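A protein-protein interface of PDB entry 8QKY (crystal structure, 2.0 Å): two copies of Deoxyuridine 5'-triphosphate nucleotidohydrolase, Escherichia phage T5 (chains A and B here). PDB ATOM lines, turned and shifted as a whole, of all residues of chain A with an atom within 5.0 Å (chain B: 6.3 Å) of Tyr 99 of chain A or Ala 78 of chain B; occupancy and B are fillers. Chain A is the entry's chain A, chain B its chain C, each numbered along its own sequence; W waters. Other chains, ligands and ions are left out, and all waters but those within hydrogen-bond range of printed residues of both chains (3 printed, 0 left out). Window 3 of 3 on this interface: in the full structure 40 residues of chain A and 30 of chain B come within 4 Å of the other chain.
The backbone carbonyl oxygen (O) of Tyr 99 of chain A lies within hydrogen-bond range of the side-chain hydroxyl (OH) of Tyr 97 of chain B, 3.5 Å away.
OH of Tyr 99 of chain A sits at hydrogen-bond distance from O of Ala 78 of chain B (2.8 Å).
Ala 78 of chain B touches Gly 71 of chain A.
Asn 79 of chain B touches Gly 71 of chain A.
His 74 of chain A touches Tyr 97 of chain B.
CB of Met 76 of chain A touches OG1 of Thr 80 of chain B, at 3.9 Å.
The backbone carbonyl oxygen (O) of Met 76 of chain B sits at hydrogen-bond distance from the backbone NH (N) of Tyr 97 of chain B, 2.7 Å away.
The backbone NH (N) of Ala 78 of chain B is in hydrogen-bond range of the backbone carbonyl oxygen (O) of Asn 95 of chain B (2.6 Å).
The backbone carbonyl oxygen of Met 76 of chain A lies within hydrogen-bond range of the backbone NH of Tyr 97 of chain A, at 2.6 Å.
O of His 74 of chain A lies close to OD1 of Asn 98 of chain A, 3.4 Å away.
The backbone carbonyl oxygen of His 74 of chain A is in hydrogen-bond range of the backbone NH of Tyr 99 of chain A (3.0 Å).
Printed residues of chain B that touch a printed residue of chain A: Ala 78, Asn 79, Thr 80 and Tyr 97.
Hydrophobic or aromatic side chains of chain B within 4 Å of the printed part of chain A: Ala 78 and Tyr 97.
Of the 11 printed residues of chain A, 4 touch a printed residue of chain B.
Printed residues of chain A that touch a printed residue of chain B: Gly 71, His 74, Met 76 and Tyr 99.
Hydrophobic or aromatic side chains of chain A within 4 Å of the printed part of chain B: His 74, Met 76 and Tyr 99.
Water W1 lies within hydrogen-bond range of the backbone carbonyl oxygen of Leu 75 of chain A, the backbone carbonyl oxygen of Ala 78 of chain B and the side-chain hydroxyl of Thr 80 of chain B.
Water W2 lies within hydrogen-bond range of OD1 of Asn 79 of chain B (2.9 Å), NZ of Lys 72 of chain A (2.9 Å) and ND2 of Asn 95 of chain B (2.9 Å).
Water W3 lies within hydrogen-bond range of OH of Tyr 97 of chain B (2.9 Å) and O of Tyr 99 of chain A (3.2 Å).
Of chain B, only Ala 78 (2.8 Å) and Tyr 97 (3.4 Å) come within 4 Å of Tyr 99 of chain A.
Ala 78 of chain B touches two residues of chain A.
Printed residues of chain A within 4 Å of Asn 79 of chain B: Gly 71 (3.6 Å).
Of the printed residues of chain B, Gly 71 of chain A touches Ala 78 and Asn 79.
Printed residues of chain A within 4 Å of Thr 80 of chain B: Met 76.
Of the printed residues of chain A, Tyr 97 of chain B touches His 74 and Tyr 99.
Ile 77 of chain B touches none of the printed residues of chain A.
Leu 75 of chain A touches none of the printed residues of chain B.
The nearest residue of chain A that does not touch Ala 78 of chain B is Leu 75 of chain A (4.3 Å).
The nearest printed residue of chain A that does not touch Asn 79 of chain B is Tyr 99 of chain A (4.7 Å).
Tyr 99 of chain A touches Tyr 97 of chain B, but with the chains exchanged Tyr 97 of chain A does not touch Tyr 99 of chain B (8.8 Å).
3 positions are printed for both chains.
Of the 6 pairs that touch across the chains among the printed residues, none has its exchanged pair printed and touching as well.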
ATOM      1  N   LEU A  70      21.825 -13.431  11.759  1.00  0.00           N
ATOM      2  CA  LEU A  70      21.347 -13.531  13.135  1.00  0.00           C
ATOM      3  C   LEU A  70      22.178 -14.508  13.953  1.00  0.00           C
ATOM      4  O   LEU A  70      22.173 -14.428  15.185  1.00  0.00           O
ATOM      5  CB  LEU A  70      19.878 -13.944  13.184  1.00  0.00           C
ATOM      6  CG  LEU A  70      18.909 -12.786  13.408  1.00  0.00           C
ATOM      7  CD1 LEU A  70      19.202 -11.661  12.417  1.00  0.00           C
ATOM      8  CD2 LEU A  70      17.427 -13.234  13.384  1.00  0.00           C
ATOM      9  N   GLY A  71      22.906 -15.418  13.300  1.00  0.00           N
ATOM     10  CA  GLY A  71      23.665 -16.399  14.051  1.00  0.00           C
ATOM     11  C   GLY A  71      24.775 -15.749  14.848  1.00  0.00           C
ATOM     12  O   GLY A  71      24.976 -16.061  16.026  1.00  0.00           O
ATOM     13  N   LYS A  72      25.483 -14.808  14.221  1.00  0.00           N
ATOM     14  CA  LYS A  72      26.504 -14.031  14.910  1.00  0.00           C
ATOM     15  C   LYS A  72      25.901 -13.216  16.043  1.00  0.00           C
ATOM     16  O   LYS A  72      26.577 -12.940  17.043  1.00  0.00           O
ATOM     17  CB  LYS A  72      27.233 -13.103  13.923  1.00  0.00           C
ATOM     18  CG  LYS A  72      27.986 -13.758  12.715  1.00  0.00           C
ATOM     19  CD  LYS A  72      27.165 -14.776  11.877  1.00  0.00           C
ATOM     20  CE  LYS A  72      27.870 -15.207  10.588  1.00  0.00           C
ATOM     21  NZ  LYS A  72      27.064 -16.278   9.892  1.00  0.00           N
ATOM     22  N   HIS A  74      23.375 -14.289  17.841  1.00  0.00           N
ATOM     23  CA  HIS A  74      22.806 -15.243  18.794  1.00  0.00           C
ATOM     24  C   HIS A  74      21.340 -14.923  19.076  1.00  0.00           C
ATOM     25  O   HIS A  74      20.875 -14.918  20.215  1.00  0.00           O
ATOM     26  CB  HIS A  74      23.633 -15.297  20.081  1.00  0.00           C
ATOM     27  CG  HIS A  74      25.013 -15.831  19.869  1.00  0.00           C
ATOM     28  ND1 HIS A  74      26.111 -15.379  20.571  1.00  0.00           N
ATOM     29  CD2 HIS A  74      25.478 -16.757  18.996  1.00  0.00           C
ATOM     30  CE1 HIS A  74      27.189 -16.018  20.152  1.00  0.00           C
ATOM     31  NE2 HIS A  74      26.833 -16.858  19.198  1.00  0.00           N
ATOM     32  N   LEU A  75      20.612 -14.656  17.995  1.00  0.00           N
ATOM     33  CA  LEU A  75      19.170 -14.503  18.014  1.00  0.00           C
ATOM     34  C   LEU A  75      18.560 -15.693  17.289  1.00  0.00           C
ATOM     35  O   LEU A  75      19.069 -16.113  16.251  1.00  0.00           O
ATOM     36  CB  LEU A  75      18.741 -13.192  17.333  1.00  0.00           C
ATOM     37  CG  LEU A  75      19.203 -11.879  17.995  1.00  0.00           C
ATOM     38  CD1 LEU A  75      18.753 -10.664  17.179  1.00  0.00           C
ATOM     39  CD2 LEU A  75      18.667 -11.789  19.404  1.00  0.00           C
ATOM     40  N   MET A  76      17.484 -16.245  17.840  1.00  0.00           N
ATOM     41  CA  MET A  76      16.743 -17.302  17.167  1.00  0.00           C
ATOM     42  C   MET A  76      15.257 -16.989  17.248  1.00  0.00           C
ATOM     43  O   MET A  76      14.817 -16.203  18.091  1.00  0.00           O
ATOM     44  CB  MET A  76      17.010 -18.679  17.796  1.00  0.00           C
ATOM     45  CG  MET A  76      16.621 -18.762  19.265  1.00  0.00           C
ATOM     46  SD  MET A  76      17.073 -20.324  20.075  1.00  0.00           S
ATOM     47  CE  MET A  76      15.646 -21.325  19.681  1.00  0.00           C
ATOM     48  N   TYR A  97      14.385 -14.588  20.121  1.00  0.00           N
ATOM     49  CA  TYR A  97      14.907 -14.871  21.449  1.00  0.00           C
ATOM     50  C   TYR A  97      16.420 -14.690  21.425  1.00  0.00           C
ATOM     51  O   TYR A  97      17.095 -15.188  20.516  1.00  0.00           O
ATOM     52  CB  TYR A  97      14.535 -16.294  21.890  1.00  0.00           C
ATOM     53  CG  TYR A  97      15.142 -16.732  23.205  1.00  0.00           C
ATOM     54  CD1 TYR A  97      14.512 -16.458  24.413  1.00  0.00           C
ATOM     55  CD2 TYR A  97      16.341 -17.437  23.234  1.00  0.00           C
ATOM     56  CE1 TYR A  97      15.066 -16.883  25.624  1.00  0.00           C
ATOM     57  CE2 TYR A  97      16.905 -17.849  24.431  1.00  0.00           C
ATOM     58  CZ  TYR A  97      16.268 -17.567  25.618  1.00  0.00           C
ATOM     59  OH  TYR A  97      16.847 -17.985  26.797  1.00  0.00           O
ATOM     60  N   ASN A  98      16.948 -13.972  22.413  1.00  0.00           N
ATOM     61  CA  ASN A  98      18.396 -13.761  22.520  1.00  0.00           C
ATOM     62  C   ASN A  98      18.975 -14.887  23.365  1.00  0.00           C
ATOM     63  O   ASN A  98      18.855 -14.876  24.593  1.00  0.00           O
ATOM     64  CB  ASN A  98      18.690 -12.404  23.144  1.00  0.00           C
ATOM     65  CG  ASN A  98      20.176 -12.097  23.215  1.00  0.00           C
ATOM     66  OD1 ASN A  98      21.030 -12.971  23.038  1.00  0.00           O
ATOM     67  ND2 ASN A  98      20.490 -10.837  23.445  1.00  0.00           N
ATOM     68  N   TYR A  99      19.620 -15.856  22.719  1.00  0.00           N
ATOM     69  CA  TYR A  99      20.189 -16.966  23.468  1.00  0.00           C
ATOM     70  C   TYR A  99      21.650 -16.745  23.818  1.00  0.00           C
ATOM     71  O   TYR A  99      22.248 -17.604  24.475  1.00  0.00           O
ATOM     72  CB  TYR A  99      20.029 -18.287  22.697  1.00  0.00           C
ATOM     73  CG  TYR A  99      20.828 -18.391  21.420  1.00  0.00           C
ATOM     74  CD1 TYR A  99      22.164 -18.770  21.436  1.00  0.00           C
ATOM     75  CD2 TYR A  99      20.243 -18.120  20.193  1.00  0.00           C
ATOM     76  CE1 TYR A  99      22.902 -18.855  20.265  1.00  0.00           C
ATOM     77  CE2 TYR A  99      20.962 -18.222  19.027  1.00  0.00           C
ATOM     78  CZ  TYR A  99      22.295 -18.589  19.069  1.00  0.00           C
ATOM     79  OH  TYR A  99      23.016 -18.674  17.903  1.00  0.00           O
ATOM     80  N   GLY A 100      22.237 -15.625  23.404  1.00  0.00           N
ATOM     81  CA  GLY A 100      23.631 -15.333  23.683  1.00  0.00           C
ATOM     82  C   GLY A 100      23.824 -14.605  24.994  1.00  0.00           C
ATOM     83  O   GLY A 100      22.944 -14.562  25.856  1.00  0.00           O
ATOM     84  N   SER A 101      25.013 -14.027  25.155  1.00  0.00           N
ATOM     85  CA  SER A 101      25.356 -13.381  26.408  1.00  0.00           C
ATOM     86  C   SER A 101      25.379 -11.864  26.309  1.00  0.00           C
ATOM     87  O   SER A 101      25.414 -11.196  27.347  1.00  0.00           O
ATOM     88  CB  SER A 101      26.723 -13.878  26.907  1.00  0.00           C
ATOM     89  OG  SER A 101      27.721 -13.639  25.937  1.00  0.00           O
ATOM     90  N   SER B  45      30.790 -20.314  19.811  1.00  0.00           N
ATOM     91  CA  SER B  45      30.494 -20.789  18.474  1.00  0.00           C
ATOM     92  C   SER B  45      31.799 -21.015  17.722  1.00  0.00           C
ATOM     93  O   SER B  45      32.852 -20.515  18.109  1.00  0.00           O
ATOM     94  CB  SER B  45      29.619 -19.791  17.723  1.00  0.00           C
ATOM     95  OG  SER B  45      30.409 -18.737  17.215  1.00  0.00           O
ATOM     96  N   MET B  76      24.037 -26.509  18.132  1.00  0.00           N
ATOM     97  CA  MET B  76      23.075 -26.084  17.128  1.00  0.00           C
ATOM     98  C   MET B  76      23.781 -25.206  16.105  1.00  0.00           C
ATOM     99  O   MET B  76      24.858 -24.660  16.365  1.00  0.00           O
ATOM    100  CB  MET B  76      21.910 -25.304  17.759  1.00  0.00           C
ATOM    101  CG  MET B  76      22.332 -24.023  18.477  1.00  0.00           C
ATOM    102  SD  MET B  76      20.893 -23.192  19.191  1.00  0.00           S
ATOM    103  CE  MET B  76      19.893 -22.861  17.740  1.00  0.00           C
ATOM    104  N   ILE B  77      23.172 -25.071  14.929  1.00  0.00           N
ATOM    105  CA  ILE B  77      23.615 -24.042  14.002  1.00  0.00           C
ATOM    106  C   ILE B  77      23.224 -22.686  14.574  1.00  0.00           C
ATOM    107  O   ILE B  77      22.063 -22.475  14.940  1.00  0.00           O
ATOM    108  CB  ILE B  77      23.003 -24.261  12.616  1.00  0.00           C
ATOM    109  CG1 ILE B  77      23.504 -25.573  12.003  1.00  0.00           C
ATOM    110  CG2 ILE B  77      23.353 -23.111  11.708  1.00  0.00           C
ATOM    111  CD1 ILE B  77      22.629 -26.032  10.800  1.00  0.00           C
ATOM    112  N   ALA B  78      24.200 -21.771  14.683  1.00  0.00           N
ATOM    113  CA  ALA B  78      23.946 -20.481  15.322  1.00  0.00           C
ATOM    114  C   ALA B  78      22.762 -19.754  14.695  1.00  0.00           C
ATOM    115  O   ALA B  78      21.954 -19.140  15.403  1.00  0.00           O
ATOM    116  CB  ALA B  78      25.195 -19.599  15.260  1.00  0.00           C
ATOM    117  N   ASN B  79      22.642 -19.805  13.372  1.00  0.00           N
ATOM    118  CA  ASN B  79      21.516 -19.210  12.664  1.00  0.00           C
ATOM    119  C   ASN B  79      20.395 -20.218  12.415  1.00  0.00           C
ATOM    120  O   ASN B  79      19.608 -20.035  11.479  1.00  0.00           O
ATOM    121  CB  ASN B  79      21.989 -18.589  11.343  1.00  0.00           C
ATOM    122  CG  ASN B  79      22.880 -19.524  10.555  1.00  0.00           C
ATOM    123  OD1 ASN B  79      23.931 -19.943  11.043  1.00  0.00           O
ATOM    124  ND2 ASN B  79      22.469 -19.862   9.331  1.00  0.00           N
ATOM    125  N   THR B  80      20.328 -21.272  13.237  1.00  0.00           N
ATOM    126  CA  THR B  80      19.256 -22.273  13.271  1.00  0.00           C
ATOM    127  C   THR B  80      19.263 -23.207  12.055  1.00  0.00           C
ATOM    128  O   THR B  80      19.303 -24.430  12.218  1.00  0.00           O
ATOM    129  CB  THR B  80      17.883 -21.600  13.434  1.00  0.00           C
ATOM    130  OG1 THR B  80      17.788 -20.966  14.722  1.00  0.00           O
ATOM    131  CG2 THR B  80      16.751 -22.642  13.330  1.00  0.00           C
ATOM    132  N   ALA B  81      19.226 -22.669  10.839  1.00  0.00           N
ATOM    133  CA  ALA B  81      19.226 -23.510   9.648  1.00  0.00           C
ATOM    134  C   ALA B  81      19.854 -22.735   8.505  1.00  0.00           C
ATOM    135  O   ALA B  81      19.517 -21.567   8.284  1.00  0.00           O
ATOM    136  CB  ALA B  81      17.805 -23.959   9.265  1.00  0.00           C
ATOM    137  N   ASN B  95      28.104 -22.780  11.160  1.00  0.00           N
ATOM    138  CA  ASN B  95      28.475 -22.013  12.348  1.00  0.00           C
ATOM    139  C   ASN B  95      27.782 -22.643  13.554  1.00  0.00           C
ATOM    140  O   ASN B  95      26.604 -22.377  13.824  1.00  0.00           O
ATOM    141  CB  ASN B  95      28.110 -20.541  12.177  1.00  0.00           C
ATOM    142  CG  ASN B  95      28.758 -19.668  13.224  1.00  0.00           C
ATOM    143  OD1 ASN B  95      29.749 -20.062  13.839  1.00  0.00           O
ATOM    144  ND2 ASN B  95      28.192 -18.488  13.452  1.00  0.00           N
ATOM    145  N   LEU B  96      28.507 -23.485  14.284  1.00  0.00           N
ATOM    146  CA  LEU B  96      27.920 -24.301  15.339  1.00  0.00           C
ATOM    147  C   LEU B  96      28.091 -23.607  16.678  1.00  0.00           C
ATOM    148  O   LEU B  96      29.178 -23.117  16.993  1.00  0.00           O
ATOM    149  CB  LEU B  96      28.566 -25.688  15.380  1.00  0.00           C
ATOM    150  CG  LEU B  96      28.352 -26.596  14.158  1.00  0.00           C
ATOM    151  CD1 LEU B  96      28.708 -28.045  14.466  1.00  0.00           C
ATOM    152  CD2 LEU B  96      26.911 -26.510  13.679  1.00  0.00           C
ATOM    153  N   TYR B  97      27.026 -23.580  17.464  1.00  0.00           N
ATOM    154  CA  TYR B  97      27.006 -22.921  18.756  1.00  0.00           C
ATOM    155  C   TYR B  97      26.755 -23.967  19.830  1.00  0.00           C
ATOM    156  O   TYR B  97      25.910 -24.848  19.658  1.00  0.00           O
ATOM    157  CB  TYR B  97      25.914 -21.844  18.786  1.00  0.00           C
ATOM    158  CG  TYR B  97      25.682 -21.248  20.147  1.00  0.00           C
ATOM    159  CD1 TYR B  97      26.482 -20.217  20.615  1.00  0.00           C
ATOM    160  CD2 TYR B  97      24.667 -21.710  20.964  1.00  0.00           C
ATOM    161  CE1 TYR B  97      26.276 -19.666  21.854  1.00  0.00           C
ATOM    162  CE2 TYR B  97      24.457 -21.162  22.216  1.00  0.00           C
ATOM    163  CZ  TYR B  97      25.268 -20.137  22.653  1.00  0.00           C
ATOM    164  OH  TYR B  97      25.070 -19.576  23.894  1.00  0.00           O
ATOM    165  N   TYR B  99      25.147 -24.769  23.029  1.00  0.00           N
ATOM    166  CA  TYR B  99      24.157 -24.335  24.005  1.00  0.00           C
ATOM    167  C   TYR B  99      24.150 -25.187  25.268  1.00  0.00           C
ATOM    168  O   TYR B  99      23.407 -24.873  26.206  1.00  0.00           O
ATOM    169  CB  TYR B  99      22.754 -24.292  23.364  1.00  0.00           C
ATOM    170  CG  TYR B  99      22.120 -25.619  22.981  1.00  0.00           C
ATOM    171  CD1 TYR B  99      21.416 -26.367  23.911  1.00  0.00           C
ATOM    172  CD2 TYR B  99      22.168 -26.083  21.666  1.00  0.00           C
ATOM    173  CE1 TYR B  99      20.806 -27.561  23.563  1.00  0.00           C
ATOM    174  CE2 TYR B  99      21.560 -27.280  21.299  1.00  0.00           C
ATOM    175  CZ  TYR B  99      20.874 -28.011  22.257  1.00  0.00           C
ATOM    176  OH  TYR B  99      20.263 -29.197  21.924  1.00  0.00           O
HETATM  177  O   HOH W   1      19.257 -18.568  14.967  1.00  0.00           O
HETATM  178  O   HOH W   2      25.784 -17.903  11.910  1.00  0.00           O
HETATM  179  O   HOH W   3      22.925 -20.535  25.592  1.00  0.00           O
